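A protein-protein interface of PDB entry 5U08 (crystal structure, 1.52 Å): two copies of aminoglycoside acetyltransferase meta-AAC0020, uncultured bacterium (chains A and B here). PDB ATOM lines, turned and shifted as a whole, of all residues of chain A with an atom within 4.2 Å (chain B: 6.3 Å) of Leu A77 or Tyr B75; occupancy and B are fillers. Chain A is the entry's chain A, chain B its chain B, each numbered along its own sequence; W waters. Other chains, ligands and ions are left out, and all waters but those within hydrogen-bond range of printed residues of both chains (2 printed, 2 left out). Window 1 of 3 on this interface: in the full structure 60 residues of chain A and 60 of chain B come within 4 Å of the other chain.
Tyr A75 touches Leu B77. Leu A77 touches Tyr B75 (CD2 to CD1, 3.8 Å). O of Glu A78 touches CD1 of Leu B51, at 3.9 Å. Gln B54 touches Glu A78. Leu B51 touches Gln A79 (CD2 to O, 3.7 Å). Tyr A80 touches Leu B51 (CB to CD2, 3.7 Å). CZ of Phe B57 touches CD2 of Tyr A80 (3.8 Å). Tyr B75 touches Tyr A80. CD2 of Tyr B90 touches OH of Tyr A80 (3.5 Å). CD1 of Leu A86 touches OH of Tyr B90, 3.2 Å away.
Of the printed residues of chain B, Gln A79 touches Leu B51. Pro A85 touches none of the printed residues of chain B. Asn B56 touches none of the printed residues of chain A. Printed residues of chain A within 4 Å of Phe B57: Tyr A80 (3.8 Å). Tyr B75 touches just these residues of chain A: Leu A77 (3.8 Å), Glu A78 (2.6 Å) and Tyr A80 (3.7 Å). Of the printed residues of chain A, Tyr B90 touches Tyr A80 and Leu A86. The nearest residue of chain B that does not touch Leu A77 is Tyr B88 (4.1 Å). The nearest residue of chain A that does not touch Tyr B75 is Gln A79 (4.1 Å).
Water W2 lies within hydrogen-bond range of OE1 of Gln B54 (2.7 Å) and OE2 of Glu A78 (2.7 Å). Water W1 lies within hydrogen-bond range of N of Glu A78, O of Val A76 and NE2 of Gln B54.
The side-chain hydroxyl of Tyr B75 lies within hydrogen-bond range of the backbone carbonyl oxygen of Glu A78 (2.6 Å). The side-chain hydroxyl (OG1) of Thr B73 is in hydrogen-bond range of the side-chain hydroxyl (OH) of Tyr A80, at 2.8 Å.
Of the 9 printed residues of chain A, 6 touch a printed residue of chain B. Of the 17 printed residues of chain B, 7 touch a printed residue of chain A. Printed residues of chain B that touch a printed residue of chain A: Leu B51, Gln B54, Phe B57, Thr B73, Tyr B75, Leu B77 and Tyr B90. Among the printed residues, no Asp or Glu carboxylate lies within 4 Å of a Lys or Arg side-chain nitrogen of the other chain.
The backbone NH of Tyr B90 lies within hydrogen-bond range of the backbone carbonyl oxygen of Thr B73. The backbone NH (N) of Leu A77 sits at hydrogen-bond distance from the backbone carbonyl oxygen (O) of Leu A86, 2.8 Å away. O of Tyr B75 lies within hydrogen-bond range of N of Tyr B88, 2.8 Å away. The side-chain amide oxygen (OD1) of Asn B56 is in hydrogen-bond range of the side-chain amide nitrogen (NE2) of Gln B54 (2.9 Å). O of Leu B86 sits at hydrogen-bond distance from N of Leu B77 (2.8 Å).
Tyr A75 touches Leu B77, and with the chains exchanged Leu A77 touches Tyr B75. 4 positions are printed for both chains. Of the 12 pairs that touch across the chains among the printed residues, 2 have their exchanged pair printed and touching as well.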
ATOM      1  N   TYR A  75      10.206  -1.431  32.971  1.00  0.00           N
ATOM      2  CA  TYR A  75      10.216  -0.092  32.367  1.00  0.00           C
ATOM      3  C   TYR A  75       9.258   0.826  33.107  1.00  0.00           C
ATOM      4  O   TYR A  75       8.128   0.426  33.424  1.00  0.00           O
ATOM      5  CB  TYR A  75       9.765  -0.169  30.899  1.00  0.00           C
ATOM      6  CG  TYR A  75      10.718  -0.913  29.966  1.00  0.00           C
ATOM      7  CD1 TYR A  75      10.577  -2.288  29.791  1.00  0.00           C
ATOM      8  CD2 TYR A  75      11.722  -0.248  29.281  1.00  0.00           C
ATOM      9  CE1 TYR A  75      11.437  -2.990  28.953  1.00  0.00           C
ATOM     10  CE2 TYR A  75      12.597  -0.944  28.426  1.00  0.00           C
ATOM     11  CZ  TYR A  75      12.433  -2.317  28.280  1.00  0.00           C
ATOM     12  OH  TYR A  75      13.281  -3.064  27.443  1.00  0.00           O
ATOM     13  N   VAL A  76       9.697   2.063  33.338  1.00  0.00           N
ATOM     14  CA  VAL A  76       8.827   3.115  33.876  1.00  0.00           C
ATOM     15  C   VAL A  76       8.044   3.747  32.733  1.00  0.00           C
ATOM     16  O   VAL A  76       8.636   4.144  31.719  1.00  0.00           O
ATOM     17  CB  VAL A  76       9.656   4.190  34.609  1.00  0.00           C
ATOM     18  CG1 VAL A  76       8.737   5.363  35.125  1.00  0.00           C
ATOM     19  CG2 VAL A  76      10.485   3.572  35.738  1.00  0.00           C
ATOM     20  N   LEU A  77       6.725   3.843  32.908  1.00  0.00           N
ATOM     21  CA  LEU A  77       5.871   4.587  31.977  1.00  0.00           C
ATOM     22  C   LEU A  77       5.270   5.751  32.760  1.00  0.00           C
ATOM     23  O   LEU A  77       4.325   5.572  33.547  1.00  0.00           O
ATOM     24  CB  LEU A  77       4.801   3.693  31.367  1.00  0.00           C
ATOM     25  CG  LEU A  77       5.282   2.344  30.836  1.00  0.00           C
ATOM     26  CD1 LEU A  77       4.072   1.546  30.391  1.00  0.00           C
ATOM     27  CD2 LEU A  77       6.198   2.563  29.648  1.00  0.00           C
ATOM     28  N   GLU A  78       5.830   6.939  32.548  1.00  0.00           N
ATOM     29  CA  GLU A  78       5.206   8.146  33.085  1.00  0.00           C
ATOM     30  C   GLU A  78       3.833   8.329  32.452  1.00  0.00           C
ATOM     31  O   GLU A  78       3.678   8.206  31.234  1.00  0.00           O
ATOM     32  CB  GLU A  78       6.100   9.350  32.795  1.00  0.00           C
ATOM     33  CG  GLU A  78       5.827  10.595  33.627  1.00  0.00           C
ATOM     34  CD  GLU A  78       6.241  10.419  35.109  1.00  0.00           C
ATOM     35  OE1 GLU A  78       5.367  10.566  35.988  1.00  0.00           O
ATOM     36  OE2 GLU A  78       7.428  10.137  35.376  1.00  0.00           O
ATOM     37  N   GLN A  79       2.841   8.646  33.276  1.00  0.00           N
ATOM     38  CA  GLN A  79       1.453   8.728  32.836  1.00  0.00           C
ATOM     39  C   GLN A  79       1.034  10.162  32.564  1.00  0.00           C
ATOM     40  O   GLN A  79       1.566  11.115  33.148  1.00  0.00           O
ATOM     41  CB  GLN A  79       0.496   8.162  33.904  1.00  0.00           C
ATOM     42  CG  GLN A  79       0.775   6.717  34.237  1.00  0.00           C
ATOM     43  CD  GLN A  79      -0.400   6.132  34.964  1.00  0.00           C
ATOM     44  OE1 GLN A  79      -1.394   5.755  34.330  1.00  0.00           O
ATOM     45  NE2 GLN A  79      -0.329   6.095  36.298  1.00  0.00           N
ATOM     46  N   TYR A  80       0.056  10.314  31.668  1.00  0.00           N
ATOM     47  CA  TYR A  80      -0.607  11.595  31.463  1.00  0.00           C
ATOM     48  C   TYR A  80      -1.953  11.640  32.182  1.00  0.00           C
ATOM     49  O   TYR A  80      -2.592  12.691  32.208  1.00  0.00           O
ATOM     50  CB  TYR A  80      -0.775  11.912  29.949  1.00  0.00           C
ATOM     51  CG  TYR A  80      -1.147  10.690  29.132  1.00  0.00           C
ATOM     52  CD1 TYR A  80      -2.500  10.355  28.934  1.00  0.00           C
ATOM     53  CD2 TYR A  80      -0.156   9.863  28.600  1.00  0.00           C
ATOM     54  CE1 TYR A  80      -2.853   9.201  28.228  1.00  0.00           C
ATOM     55  CE2 TYR A  80      -0.490   8.716  27.883  1.00  0.00           C
ATOM     56  CZ  TYR A  80      -1.840   8.417  27.678  1.00  0.00           C
ATOM     57  OH  TYR A  80      -2.165   7.295  26.968  1.00  0.00           O
ATOM     58  N   PRO A  85       3.614   7.267  38.352  1.00  0.00           N
ATOM     59  CA  PRO A  85       3.907   6.431  37.182  1.00  0.00           C
ATOM     60  C   PRO A  85       3.403   4.995  37.309  1.00  0.00           C
ATOM     61  O   PRO A  85       2.964   4.517  38.361  1.00  0.00           O
ATOM     62  CB  PRO A  85       5.437   6.452  37.075  1.00  0.00           C
ATOM     63  CG  PRO A  85       5.880   7.604  37.940  1.00  0.00           C
ATOM     64  CD  PRO A  85       4.841   7.752  39.010  1.00  0.00           C
ATOM     65  N   LEU A  86       3.502   4.298  36.178  1.00  0.00           N
ATOM     66  CA  LEU A  86       3.293   2.862  36.070  1.00  0.00           C
ATOM     67  C   LEU A  86       4.638   2.199  35.874  1.00  0.00           C
ATOM     68  O   LEU A  86       5.539   2.775  35.265  1.00  0.00           O
ATOM     69  CB  LEU A  86       2.425   2.517  34.845  1.00  0.00           C
ATOM     70  CG  LEU A  86       1.033   3.103  34.777  1.00  0.00           C
ATOM     71  CD1 LEU A  86       0.413   2.708  33.419  1.00  0.00           C
ATOM     72  CD2 LEU A  86       0.194   2.635  35.961  1.00  0.00           C
ATOM     73  N   PHE A 124       2.531  -3.729  36.393  1.00  0.00           N
ATOM     74  CA  PHE A 124       1.829  -4.790  35.689  1.00  0.00           C
ATOM     75  C   PHE A 124       2.805  -5.710  34.986  1.00  0.00           C
ATOM     76  O   PHE A 124       3.956  -5.364  34.755  1.00  0.00           O
ATOM     77  CB  PHE A 124       0.770  -4.242  34.699  1.00  0.00           C
ATOM     78  CG  PHE A 124       1.322  -3.402  33.540  1.00  0.00           C
ATOM     79  CD1 PHE A 124       1.569  -3.970  32.315  1.00  0.00           C
ATOM     80  CD2 PHE A 124       1.502  -2.043  33.692  1.00  0.00           C
ATOM     81  CE1 PHE A 124       2.029  -3.178  31.231  1.00  0.00           C
ATOM     82  CE2 PHE A 124       1.967  -1.259  32.627  1.00  0.00           C
ATOM     83  CZ  PHE A 124       2.220  -1.841  31.406  1.00  0.00           C
ATOM     84  N   LEU B  51       6.409  15.363  30.584  1.00  0.00           N
ATOM     85  CA  LEU B  51       6.212  14.128  29.824  1.00  0.00           C
ATOM     86  C   LEU B  51       6.381  14.370  28.330  1.00  0.00           C
ATOM     87  O   LEU B  51       7.091  13.615  27.643  1.00  0.00           O
ATOM     88  CB  LEU B  51       4.837  13.545  30.142  1.00  0.00           C
ATOM     89  CG  LEU B  51       4.369  12.328  29.340  1.00  0.00           C
ATOM     90  CD1 LEU B  51       5.372  11.164  29.417  1.00  0.00           C
ATOM     91  CD2 LEU B  51       2.963  11.895  29.814  1.00  0.00           C
ATOM     92  N   GLN B  54       9.932  14.308  27.151  1.00  0.00           N
ATOM     93  CA  GLN B  54      10.737  13.094  27.235  1.00  0.00           C
ATOM     94  C   GLN B  54      11.122  12.587  25.849  1.00  0.00           C
ATOM     95  O   GLN B  54      10.334  12.652  24.901  1.00  0.00           O
ATOM     96  CB  GLN B  54       9.956  12.016  27.984  1.00  0.00           C
ATOM     97  CG  GLN B  54       9.866  12.317  29.456  1.00  0.00           C
ATOM     98  CD  GLN B  54       9.101  11.261  30.246  1.00  0.00           C
ATOM     99  OE1 GLN B  54       8.596  11.543  31.324  1.00  0.00           O
ATOM    100  NE2 GLN B  54       9.021  10.044  29.716  1.00  0.00           N
ATOM    101  N   ASN B  56      11.412   9.570  24.972  1.00  0.00           N
ATOM    102  CA  ASN B  56      10.921   8.196  24.821  1.00  0.00           C
ATOM    103  C   ASN B  56       9.400   8.151  24.743  1.00  0.00           C
ATOM    104  O   ASN B  56       8.790   7.096  24.976  1.00  0.00           O
ATOM    105  CB  ASN B  56      11.411   7.326  25.981  1.00  0.00           C
ATOM    106  CG  ASN B  56      10.729   7.682  27.276  1.00  0.00           C
ATOM    107  OD1 ASN B  56      10.307   8.818  27.430  1.00  0.00           O
ATOM    108  ND2 ASN B  56      10.548   6.702  28.200  1.00  0.00           N
ATOM    109  N   PHE B  57       8.781   9.267  24.354  1.00  0.00           N
ATOM    110  CA  PHE B  57       7.339   9.421  24.368  1.00  0.00           C
ATOM    111  C   PHE B  57       6.941  10.259  23.169  1.00  0.00           C
ATOM    112  O   PHE B  57       7.474  11.359  22.973  1.00  0.00           O
ATOM    113  CB  PHE B  57       6.886  10.134  25.661  1.00  0.00           C
ATOM    114  CG  PHE B  57       5.400  10.270  25.801  1.00  0.00           C
ATOM    115  CD1 PHE B  57       4.818  11.521  25.720  1.00  0.00           C
ATOM    116  CD2 PHE B  57       4.600   9.176  26.016  1.00  0.00           C
ATOM    117  CE1 PHE B  57       3.438  11.684  25.890  1.00  0.00           C
ATOM    118  CE2 PHE B  57       3.232   9.299  26.165  1.00  0.00           C
ATOM    119  CZ  PHE B  57       2.638  10.576  26.109  1.00  0.00           C
ATOM    120  N   TYR B  58       6.006   9.733  22.375  1.00  0.00           N
ATOM    121  CA  TYR B  58       5.571  10.393  21.145  1.00  0.00           C
ATOM    122  C   TYR B  58       4.058  10.312  21.012  1.00  0.00           C
ATOM    123  O   TYR B  58       3.451   9.237  21.163  1.00  0.00           O
ATOM    124  CB  TYR B  58       6.224   9.749  19.918  1.00  0.00           C
ATOM    125  CG  TYR B  58       7.669  10.055  19.723  1.00  0.00           C
ATOM    126  CD1 TYR B  58       8.090  11.303  19.274  1.00  0.00           C
ATOM    127  CD2 TYR B  58       8.611   9.076  19.990  1.00  0.00           C
ATOM    128  CE1 TYR B  58       9.453  11.563  19.078  1.00  0.00           C
ATOM    129  CE2 TYR B  58       9.975   9.316  19.811  1.00  0.00           C
ATOM    130  CZ  TYR B  58      10.373  10.572  19.356  1.00  0.00           C
ATOM    131  OH  TYR B  58      11.705  10.824  19.152  1.00  0.00           O
ATOM    132  N   THR B  73      -1.015   7.725  21.852  1.00  0.00           N
ATOM    133  CA  THR B  73       0.211   7.938  22.597  1.00  0.00           C
ATOM    134  C   THR B  73       1.081   6.702  22.460  1.00  0.00           C
ATOM    135  O   THR B  73       0.553   5.594  22.323  1.00  0.00           O
ATOM    136  CB  THR B  73      -0.088   8.167  24.063  1.00  0.00           C
ATOM    137  OG1 THR B  73      -0.867   7.042  24.519  1.00  0.00           O
ATOM    138  CG2 THR B  73      -0.936   9.439  24.243  1.00  0.00           C
ATOM    139  N   SER B  74       2.393   6.894  22.526  1.00  0.00           N
ATOM    140  CA  SER B  74       3.310   5.757  22.374  1.00  0.00           C
ATOM    141  C   SER B  74       4.580   5.969  23.174  1.00  0.00           C
ATOM    142  O   SER B  74       5.062   7.089  23.337  1.00  0.00           O
ATOM    143  CB  SER B  74       3.639   5.530  20.896  1.00  0.00           C
ATOM    144  OG  SER B  74       4.320   6.646  20.285  1.00  0.00           O
ATOM    145  N   TYR B  75       5.132   4.860  23.667  1.00  0.00           N
ATOM    146  CA  TYR B  75       6.339   4.848  24.487  1.00  0.00           C
ATOM    147  C   TYR B  75       7.415   4.065  23.754  1.00  0.00           C
ATOM    148  O   TYR B  75       7.137   2.963  23.272  1.00  0.00           O
ATOM    149  CB  TYR B  75       6.070   4.176  25.853  1.00  0.00           C
ATOM    150  CG  TYR B  75       5.116   4.935  26.757  1.00  0.00           C
ATOM    151  CD1 TYR B  75       5.600   5.830  27.710  1.00  0.00           C
ATOM    152  CD2 TYR B  75       3.766   4.754  26.655  1.00  0.00           C
ATOM    153  CE1 TYR B  75       4.731   6.508  28.551  1.00  0.00           C
ATOM    154  CE2 TYR B  75       2.862   5.449  27.513  1.00  0.00           C
ATOM    155  CZ  TYR B  75       3.373   6.316  28.440  1.00  0.00           C
ATOM    156  OH  TYR B  75       2.486   7.010  29.264  1.00  0.00           O
ATOM    157  N   VAL B  76       8.620   4.620  23.691  1.00  0.00           N
ATOM    158  CA  VAL B  76       9.794   3.880  23.203  1.00  0.00           C
ATOM    159  C   VAL B  76      10.308   2.962  24.297  1.00  0.00           C
ATOM    160  O   VAL B  76      10.556   3.419  25.423  1.00  0.00           O
ATOM    161  CB  VAL B  76      10.890   4.860  22.786  1.00  0.00           C
ATOM    162  CG1 VAL B  76      12.141   4.088  22.319  1.00  0.00           C
ATOM    163  CG2 VAL B  76      10.352   5.744  21.674  1.00  0.00           C
ATOM    164  N   LEU B  77      10.521   1.680  23.964  1.00  0.00           N
ATOM    165  CA  LEU B  77      11.131   0.708  24.884  1.00  0.00           C
ATOM    166  C   LEU B  77      12.427   0.244  24.228  1.00  0.00           C
ATOM    167  O   LEU B  77      12.396  -0.572  23.300  1.00  0.00           O
ATOM    168  CB  LEU B  77      10.197  -0.465  25.169  1.00  0.00           C
ATOM    169  CG  LEU B  77       8.782  -0.160  25.667  1.00  0.00           C
ATOM    170  CD1 LEU B  77       7.976  -1.465  25.836  1.00  0.00           C
ATOM    171  CD2 LEU B  77       8.776   0.643  26.991  1.00  0.00           C
ATOM    172  N   LEU B  86      11.605  -0.989  20.380  1.00  0.00           N
ATOM    173  CA  LEU B  86      10.177  -1.255  20.264  1.00  0.00           C
ATOM    174  C   LEU B  86       9.409   0.025  20.562  1.00  0.00           C
ATOM    175  O   LEU B  86       9.872   0.874  21.329  1.00  0.00           O
ATOM    176  CB  LEU B  86       9.677  -2.296  21.287  1.00  0.00           C
ATOM    177  CG  LEU B  86      10.293  -3.669  21.327  1.00  0.00           C
ATOM    178  CD1 LEU B  86       9.675  -4.404  22.518  1.00  0.00           C
ATOM    179  CD2 LEU B  86      10.062  -4.402  20.000  1.00  0.00           C
ATOM    180  N   ALA B  87       8.238   0.169  19.945  1.00  0.00           N
ATOM    181  CA  ALA B  87       7.294   1.195  20.370  1.00  0.00           C
ATOM    182  C   ALA B  87       6.014   0.542  20.859  1.00  0.00           C
ATOM    183  O   ALA B  87       5.461  -0.351  20.194  1.00  0.00           O
ATOM    184  CB  ALA B  87       6.978   2.176  19.243  1.00  0.00           C
ATOM    185  N   TYR B  88       5.516   1.038  21.988  1.00  0.00           N
ATOM    186  CA  TYR B  88       4.289   0.558  22.625  1.00  0.00           C
ATOM    187  C   TYR B  88       3.233   1.648  22.442  1.00  0.00           C
ATOM    188  O   TYR B  88       3.334   2.712  23.067  1.00  0.00           O
ATOM    189  CB  TYR B  88       4.574   0.302  24.107  1.00  0.00           C
ATOM    190  CG  TYR B  88       3.453  -0.141  25.008  1.00  0.00           C
ATOM    191  CD1 TYR B  88       2.225  -0.571  24.527  1.00  0.00           C
ATOM    192  CD2 TYR B  88       3.673  -0.229  26.379  1.00  0.00           C
ATOM    193  CE1 TYR B  88       1.207  -1.008  25.395  1.00  0.00           C
ATOM    194  CE2 TYR B  88       2.658  -0.656  27.244  1.00  0.00           C
ATOM    195  CZ  TYR B  88       1.456  -1.052  26.738  1.00  0.00           C
ATOM    196  OH  TYR B  88       0.441  -1.475  27.565  1.00  0.00           O
ATOM    197  N   ILE B  89       2.220   1.393  21.607  1.00  0.00           N
ATOM    198  CA  ILE B  89       1.067   2.299  21.521  1.00  0.00           C
ATOM    199  C   ILE B  89       0.180   2.029  22.727  1.00  0.00           C
ATOM    200  O   ILE B  89      -0.343   0.917  22.893  1.00  0.00           O
ATOM    201  CB  ILE B  89       0.274   2.099  20.222  1.00  0.00           C
ATOM    202  CG1 ILE B  89       1.123   2.434  18.994  1.00  0.00           C
ATOM    203  CG2 ILE B  89      -1.022   2.939  20.253  1.00  0.00           C
ATOM    204  CD1 ILE B  89       0.451   1.986  17.714  1.00  0.00           C
ATOM    205  N   TYR B  90       0.041   3.035  23.587  1.00  0.00           N
ATOM    206  CA  TYR B  90      -0.625   2.826  24.859  1.00  0.00           C
ATOM    207  C   TYR B  90      -2.112   3.153  24.804  1.00  0.00           C
ATOM    208  O   TYR B  90      -2.928   2.382  25.331  1.00  0.00           O
ATOM    209  CB  TYR B  90       0.091   3.648  25.936  1.00  0.00           C
ATOM    210  CG  TYR B  90      -0.371   3.278  27.309  1.00  0.00           C
ATOM    211  CD1 TYR B  90       0.177   2.189  27.973  1.00  0.00           C
ATOM    212  CD2 TYR B  90      -1.392   3.993  27.916  1.00  0.00           C
ATOM    213  CE1 TYR B  90      -0.284   1.840  29.242  1.00  0.00           C
ATOM    214  CE2 TYR B  90      -1.849   3.658  29.170  1.00  0.00           C
ATOM    215  CZ  TYR B  90      -1.298   2.586  29.816  1.00  0.00           C
ATOM    216  OH  TYR B  90      -1.780   2.283  31.065  1.00  0.00           O
ATOM    217  N   TYR B 115       8.160   5.244  13.123  1.00  0.00           N
ATOM    218  CA  TYR B 115       9.072   4.352  13.802  1.00  0.00           C
ATOM    219  C   TYR B 115       9.877   3.520  12.827  1.00  0.00           C
ATOM    220  O   TYR B 115      11.005   3.142  13.141  1.00  0.00           O
ATOM    221  CB  TYR B 115       8.277   3.490  14.803  1.00  0.00           C
ATOM    222  CG  TYR B 115       7.926   4.273  16.044  1.00  0.00           C
ATOM    223  CD1 TYR B 115       8.927   4.832  16.833  1.00  0.00           C
ATOM    224  CD2 TYR B 115       6.579   4.444  16.435  1.00  0.00           C
ATOM    225  CE1 TYR B 115       8.610   5.551  18.010  1.00  0.00           C
ATOM    226  CE2 TYR B 115       6.257   5.149  17.628  1.00  0.00           C
ATOM    227  CZ  TYR B 115       7.292   5.679  18.383  1.00  0.00           C
ATOM    228  OH  TYR B 115       6.928   6.338  19.554  1.00  0.00           O
ATOM    229  N   PHE B 120      13.145   1.303  14.130  1.00  0.00           N
ATOM    230  CA  PHE B 120      12.629   0.417  15.168  1.00  0.00           C
ATOM    231  C   PHE B 120      12.363  -0.985  14.601  1.00  0.00           C
ATOM    232  O   PHE B 120      12.195  -1.179  13.388  1.00  0.00           O
ATOM    233  CB  PHE B 120      11.334   0.980  15.752  1.00  0.00           C
ATOM    234  CG  PHE B 120      11.528   2.073  16.780  1.00  0.00           C
ATOM    235  CD1 PHE B 120      12.504   3.053  16.623  1.00  0.00           C
ATOM    236  CD2 PHE B 120      10.730   2.090  17.937  1.00  0.00           C
ATOM    237  CE1 PHE B 120      12.659   4.085  17.569  1.00  0.00           C
ATOM    238  CE2 PHE B 120      10.865   3.111  18.895  1.00  0.00           C
ATOM    239  CZ  PHE B 120      11.831   4.095  18.734  1.00  0.00           C
HETATM  240  O   HOH W   1       8.436   7.222  31.043  1.00  0.00           O
HETATM  241  O   HOH W   2       9.426  10.530  33.644  1.00  0.00           O
